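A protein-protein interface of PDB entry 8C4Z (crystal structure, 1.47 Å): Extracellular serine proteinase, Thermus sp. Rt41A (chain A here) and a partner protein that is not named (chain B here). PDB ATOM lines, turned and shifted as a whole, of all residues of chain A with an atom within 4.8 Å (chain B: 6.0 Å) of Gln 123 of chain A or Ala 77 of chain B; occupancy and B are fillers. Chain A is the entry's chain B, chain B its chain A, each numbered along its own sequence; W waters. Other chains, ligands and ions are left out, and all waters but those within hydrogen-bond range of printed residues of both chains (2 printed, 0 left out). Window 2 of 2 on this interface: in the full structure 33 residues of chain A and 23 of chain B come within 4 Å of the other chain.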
ATOM      1  N   ASP A 119      23.545 -10.342  19.491  1.00  0.00           N
ATOM      2  CA  ASP A 119      22.867 -10.741  18.261  1.00  0.00           C
ATOM      3  C   ASP A 119      23.874 -11.191  17.215  1.00  0.00           C
ATOM      4  O   ASP A 119      23.688 -12.233  16.560  1.00  0.00           O
ATOM      5  CB  ASP A 119      22.031  -9.568  17.733  1.00  0.00           C
ATOM      6  CG  ASP A 119      21.059  -9.988  16.642  1.00  0.00           C
ATOM      7  OD1 ASP A 119      20.223 -10.874  16.915  1.00  0.00           O
ATOM      8  OD2 ASP A 119      21.124  -9.429  15.517  1.00  0.00           O
ATOM      9  N   TRP A 120      24.961 -10.423  17.052  1.00  0.00           N
ATOM     10  CA  TRP A 120      25.991 -10.786  16.086  1.00  0.00           C
ATOM     11  C   TRP A 120      26.623 -12.133  16.421  1.00  0.00           C
ATOM     12  O   TRP A 120      26.804 -12.979  15.537  1.00  0.00           O
ATOM     13  CB  TRP A 120      27.056  -9.694  15.995  1.00  0.00           C
ATOM     14  CG  TRP A 120      28.067  -9.980  14.925  1.00  0.00           C
ATOM     15  CD1 TRP A 120      27.994  -9.627  13.611  1.00  0.00           C
ATOM     16  CD2 TRP A 120      29.301 -10.692  15.082  1.00  0.00           C
ATOM     17  NE1 TRP A 120      29.110 -10.068  12.935  1.00  0.00           N
ATOM     18  CE2 TRP A 120      29.925 -10.732  13.817  1.00  0.00           C
ATOM     19  CE3 TRP A 120      29.942 -11.289  16.172  1.00  0.00           C
ATOM     20  CZ2 TRP A 120      31.159 -11.347  13.615  1.00  0.00           C
ATOM     21  CZ3 TRP A 120      31.161 -11.900  15.972  1.00  0.00           C
ATOM     22  CH2 TRP A 120      31.758 -11.927  14.698  1.00  0.00           C
ATOM     23  N   VAL A 121      26.988 -12.344  17.695  1.00  0.00           N
ATOM     24  CA  VAL A 121      27.586 -13.622  18.083  1.00  0.00           C
ATOM     25  C   VAL A 121      26.606 -14.768  17.872  1.00  0.00           C
ATOM     26  O   VAL A 121      26.984 -15.841  17.382  1.00  0.00           O
ATOM     27  CB  VAL A 121      28.112 -13.593  19.535  1.00  0.00           C
ATOM     28  CG1 VAL A 121      28.725 -14.964  19.884  1.00  0.00           C
ATOM     29  CG2 VAL A 121      29.152 -12.508  19.706  1.00  0.00           C
ATOM     30  N   THR A 122      25.344 -14.586  18.280  1.00  0.00           N
ATOM     31  CA  THR A 122      24.383 -15.678  18.133  1.00  0.00           C
ATOM     32  C   THR A 122      24.263 -16.089  16.668  1.00  0.00           C
ATOM     33  O   THR A 122      24.235 -17.287  16.340  1.00  0.00           O
ATOM     34  CB  THR A 122      23.027 -15.261  18.726  1.00  0.00           C
ATOM     35  OG1 THR A 122      23.197 -14.959  20.122  1.00  0.00           O
ATOM     36  CG2 THR A 122      22.016 -16.384  18.599  1.00  0.00           C
ATOM     37  N   GLN A 123      24.243 -15.103  15.773  1.00  0.00           N
ATOM     38  CA  GLN A 123      24.134 -15.366  14.343  1.00  0.00           C
ATOM     39  C   GLN A 123      25.412 -15.972  13.770  1.00  0.00           C
ATOM     40  O   GLN A 123      25.351 -16.919  12.976  1.00  0.00           O
ATOM     41  CB  GLN A 123      23.767 -14.064  13.627  1.00  0.00           C
ATOM     42  CG  GLN A 123      23.812 -14.168  12.106  1.00  0.00           C
ATOM     43  CD  GLN A 123      22.598 -14.848  11.533  1.00  0.00           C
ATOM     44  OE1 GLN A 123      21.640 -15.141  12.248  1.00  0.00           O
ATOM     45  NE2 GLN A 123      22.629 -15.110  10.229  1.00  0.00           N
ATOM     46  N   ASN A 124      26.581 -15.451  14.153  1.00  0.00           N
ATOM     47  CA  ASN A 124      27.803 -15.697  13.398  1.00  0.00           C
ATOM     48  C   ASN A 124      28.868 -16.496  14.137  1.00  0.00           C
ATOM     49  O   ASN A 124      29.955 -16.699  13.583  1.00  0.00           O
ATOM     50  CB  ASN A 124      28.399 -14.366  12.938  1.00  0.00           C
ATOM     51  CG  ASN A 124      27.474 -13.624  12.011  1.00  0.00           C
ATOM     52  OD1 ASN A 124      27.193 -14.083  10.895  1.00  0.00           O
ATOM     53  ND2 ASN A 124      26.982 -12.477  12.462  1.00  0.00           N
ATOM     54  N   HIS A 125      28.613 -16.944  15.362  1.00  0.00           N
ATOM     55  CA  HIS A 125      29.660 -17.654  16.079  1.00  0.00           C
ATOM     56  C   HIS A 125      30.016 -18.949  15.359  1.00  0.00           C
ATOM     57  O   HIS A 125      29.227 -19.497  14.584  1.00  0.00           O
ATOM     58  CB  HIS A 125      29.194 -17.999  17.485  1.00  0.00           C
ATOM     59  CG  HIS A 125      28.143 -19.062  17.522  1.00  0.00           C
ATOM     60  ND1 HIS A 125      26.799 -18.783  17.361  1.00  0.00           N
ATOM     61  CD2 HIS A 125      28.237 -20.409  17.664  1.00  0.00           C
ATOM     62  CE1 HIS A 125      26.112 -19.911  17.438  1.00  0.00           C
ATOM     63  NE2 HIS A 125      26.962 -20.912  17.611  1.00  0.00           N
ATOM     64  N   ASN A 149      18.904 -16.446  24.626  1.00  0.00           N
ATOM     65  CA  ASN A 149      18.862 -16.926  23.253  1.00  0.00           C
ATOM     66  C   ASN A 149      20.249 -17.312  22.740  1.00  0.00           C
ATOM     67  O   ASN A 149      20.374 -18.265  21.959  1.00  0.00           O
ATOM     68  CB  ASN A 149      18.140 -15.917  22.362  1.00  0.00           C
ATOM     69  CG  ASN A 149      16.639 -15.923  22.592  1.00  0.00           C
ATOM     70  OD1 ASN A 149      16.078 -16.923  23.041  1.00  0.00           O
ATOM     71  ND2 ASN A 149      15.980 -14.816  22.280  1.00  0.00           N
ATOM     72  N   GLU B  40      15.319  -8.871   8.904  1.00  0.00           N
ATOM     73  CA  GLU B  40      16.497  -9.313   8.158  1.00  0.00           C
ATOM     74  C   GLU B  40      16.828  -8.332   7.038  1.00  0.00           C
ATOM     75  O   GLU B  40      18.003  -8.058   6.771  1.00  0.00           O
ATOM     76  CB  GLU B  40      16.300 -10.735   7.606  1.00  0.00           C
ATOM     77  CG  GLU B  40      16.159 -11.801   8.702  1.00  0.00           C
ATOM     78  CD  GLU B  40      17.492 -12.284   9.271  1.00  0.00           C
ATOM     79  OE1 GLU B  40      17.484 -13.246  10.068  1.00  0.00           O
ATOM     80  OE2 GLU B  40      18.548 -11.715   8.917  1.00  0.00           O
ATOM     81  N   LYS B  43      18.445  -5.229   8.721  1.00  0.00           N
ATOM     82  CA  LYS B  43      19.826  -5.520   9.087  1.00  0.00           C
ATOM     83  C   LYS B  43      20.732  -5.503   7.861  1.00  0.00           C
ATOM     84  O   LYS B  43      21.829  -4.931   7.896  1.00  0.00           O
ATOM     85  CB  LYS B  43      19.925  -6.862   9.819  1.00  0.00           C
ATOM     86  CG  LYS B  43      21.323  -7.142  10.361  1.00  0.00           C
ATOM     87  CD  LYS B  43      21.467  -8.574  10.875  1.00  0.00           C
ATOM     88  CE  LYS B  43      20.739  -8.806  12.165  1.00  0.00           C
ATOM     89  NZ  LYS B  43      21.260 -10.046  12.834  1.00  0.00           N
ATOM     90  N   TYR B  75      17.690  -6.481  15.506  1.00  0.00           N
ATOM     91  CA  TYR B  75      17.984  -7.757  16.137  1.00  0.00           C
ATOM     92  C   TYR B  75      17.143  -8.848  15.504  1.00  0.00           C
ATOM     93  O   TYR B  75      15.923  -8.683  15.348  1.00  0.00           O
ATOM     94  CB  TYR B  75      17.673  -7.698  17.631  1.00  0.00           C
ATOM     95  CG  TYR B  75      18.236  -6.474  18.322  1.00  0.00           C
ATOM     96  CD1 TYR B  75      19.603  -6.195  18.288  1.00  0.00           C
ATOM     97  CD2 TYR B  75      17.395  -5.599  19.029  1.00  0.00           C
ATOM     98  CE1 TYR B  75      20.123  -5.075  18.932  1.00  0.00           C
ATOM     99  CE2 TYR B  75      17.907  -4.488  19.679  1.00  0.00           C
ATOM    100  CZ  TYR B  75      19.266  -4.229  19.632  1.00  0.00           C
ATOM    101  OH  TYR B  75      19.757  -3.115  20.275  1.00  0.00           O
ATOM    102  N   THR B  76      17.790  -9.968  15.160  1.00  0.00           N
ATOM    103  CA  THR B  76      17.073 -11.083  14.551  1.00  0.00           C
ATOM    104  C   THR B  76      17.345 -12.405  15.258  1.00  0.00           C
ATOM    105  O   THR B  76      16.515 -13.318  15.201  1.00  0.00           O
ATOM    106  CB  THR B  76      17.445 -11.244  13.073  1.00  0.00           C
ATOM    107  OG1 THR B  76      18.853 -11.483  12.960  1.00  0.00           O
ATOM    108  CG2 THR B  76      17.070  -9.986  12.274  1.00  0.00           C
ATOM    109  N   ALA B  77      18.501 -12.538  15.907  1.00  0.00           N
ATOM    110  CA  ALA B  77      18.962 -13.836  16.394  1.00  0.00           C
ATOM    111  C   ALA B  77      18.936 -13.960  17.909  1.00  0.00           C
ATOM    112  O   ALA B  77      18.409 -14.942  18.449  1.00  0.00           O
ATOM    113  CB  ALA B  77      20.376 -14.128  15.867  1.00  0.00           C
ATOM    114  N   ALA B  78      19.503 -12.994  18.618  1.00  0.00           N
ATOM    115  CA  ALA B  78      19.402 -12.986  20.070  1.00  0.00           C
ATOM    116  C   ALA B  78      18.051 -12.470  20.547  1.00  0.00           C
ATOM    117  O   ALA B  78      17.689 -12.679  21.710  1.00  0.00           O
ATOM    118  CB  ALA B  78      20.540 -12.147  20.655  1.00  0.00           C
ATOM    119  N   LEU B  79      17.281 -11.855  19.659  1.00  0.00           N
ATOM    120  CA  LEU B  79      16.055 -11.149  19.975  1.00  0.00           C
ATOM    121  C   LEU B  79      15.449 -10.762  18.638  1.00  0.00           C
ATOM    122  O   LEU B  79      16.175 -10.635  17.650  1.00  0.00           O
ATOM    123  CB  LEU B  79      16.402  -9.874  20.761  1.00  0.00           C
ATOM    124  CG  LEU B  79      15.357  -9.218  21.646  1.00  0.00           C
ATOM    125  CD1 LEU B  79      14.913 -10.160  22.735  1.00  0.00           C
ATOM    126  CD2 LEU B  79      15.931  -7.949  22.247  1.00  0.00           C
ATOM    127  N   ARG B  80      14.116 -10.600  18.600  1.00  0.00           N
ATOM    128  CA  ARG B  80      13.430  -9.973  17.462  1.00  0.00           C
ATOM    129  C   ARG B  80      13.041  -8.562  17.895  1.00  0.00           C
ATOM    130  O   ARG B  80      12.152  -8.389  18.734  1.00  0.00           O
ATOM    131  CB  ARG B  80      12.191 -10.764  17.033  1.00  0.00           C
ATOM    132  CG  ARG B  80      12.451 -11.943  16.087  1.00  0.00           C
ATOM    133  CD  ARG B  80      13.576 -12.808  16.584  1.00  0.00           C
ATOM    134  NE  ARG B  80      13.254 -13.441  17.853  1.00  0.00           N
ATOM    135  CZ  ARG B  80      14.086 -14.233  18.513  1.00  0.00           C
ATOM    136  NH1 ARG B  80      15.298 -14.494  18.051  1.00  0.00           N
ATOM    137  NH2 ARG B  80      13.706 -14.749  19.680  1.00  0.00           N
HETATM  138  O   HOH W   1      12.873 -14.648  22.591  1.00  0.00           O
HETATM  139  O   HOH W   2      19.082 -14.060  12.042  1.00  0.00           O
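Water W2 lies within hydrogen-bond range of the side-chain carboxylate (OE1) of Glu 40 of chain B (2.7 Å), the side-chain hydroxyl (OG1) of Thr 76 of chain B (2.7 Å) and the side-chain amide oxygen (OE1) of Gln 123 of chain A (2.8 Å). Water W1 lies within hydrogen-bond range of NH2 of Arg 80 of chain B (3.0 Å) and ND2 of Asn 149 of chain A (3.1 Å).
The side-chain amino group (NZ) of Lys 43 of chain B sits at hydrogen-bond distance from the side-chain hydroxyl (OG1) of Thr 76 of chain B, at 2.8 Å. O of Thr 76 of chain B lies close to NH1 of Arg 80 of chain B (3.3 Å). The backbone carbonyl oxygen of Ala 77 of chain B lies within hydrogen-bond range of the guanidinium group of Arg 80 of chain B. The backbone carbonyl oxygen of Thr 122 of chain A is in hydrogen-bond range of a ring nitrogen (ND1) of His 125 of chain A (3.1 Å).
OD2 of Asp 119 of chain A touches CA of Tyr 75 of chain B, at 3.6 Å. Ala 77 of chain B touches Thr 122 of chain A (O to CG2, 3.9 Å). OG1 of Thr 122 of chain A touches CB of Ala 78 of chain B, at 3.9 Å. Gln 123 of chain A touches Ala 77 of chain B (OE1 to CB, 3.96 Å).
The side-chain amino group (NZ) of Lys 43 of chain B lies within salt-bridge range of the side-chain carboxylate (OD2) of Asp 119 of chain A (2.8 Å). N of Thr 76 of chain B lies within hydrogen-bond range of OD1 of Asp 119 of chain A, at 3.1 Å. The backbone NH (N) of Ala 77 of chain B sits at hydrogen-bond distance from the side-chain carboxylate (OD1) of Asp 119 of chain A, at 2.6 Å. OD1 of Asp 119 of chain A lies within hydrogen-bond range of N of Ala 78 of chain B (2.8 Å). ND2 of Asn 149 of chain A lies within hydrogen-bond range of O of Ala 78 of chain B, 2.8 Å away. The side-chain amide nitrogen (ND2) of Asn 149 of chain A sits close to the guanidinium group (NH2) of Arg 80 of chain B.
Of the 8 printed residues of chain B, 6 touch a printed residue of chain A. Along chain B the printed residues that touch a printed residue of chain A span positions 43 to 80. Of the 8 printed residues of chain A, 4 touch a printed residue of chain B. Among the printed residues, Asp or Glu carboxylates within 4 Å of a Lys or Arg side-chain nitrogen of the other chain: Asp 119 of chain A with Lys 43 of chain B.
Printed residues of chain B within 4 Å of Asp 119 of chain A: Lys 43 (2.8 Å), Tyr 75 (3.6 Å), Thr 76 (3.1 Å), Ala 77 (2.6 Å) and Ala 78 (2.8 Å). Printed residues of chain B within 4 Å of Thr 122 of chain A: Ala 77 (3.9 Å) and Ala 78 (3.9 Å). Of chain B, only Ala 77 comes within 4 Å of Gln 123 of chain A. Asn 124 of chain A touches none of the printed residues of chain B. Glu 40 of chain B touches none of the printed residues of chain A. Printed residues of chain A within 4 Å of Lys 43 of chain B: Asp 119 (2.8 Å). Printed residues of chain A within 4 Å of Thr 76 of chain B: Asp 119. Of chain A, only Asp 119, Thr 122 and Gln 123 come within 4 Å of Ala 77 of chain B. The nearest printed residue of chain A that does not touch Tyr 75 of chain B is Trp 120 of chain A (6.9 Å).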
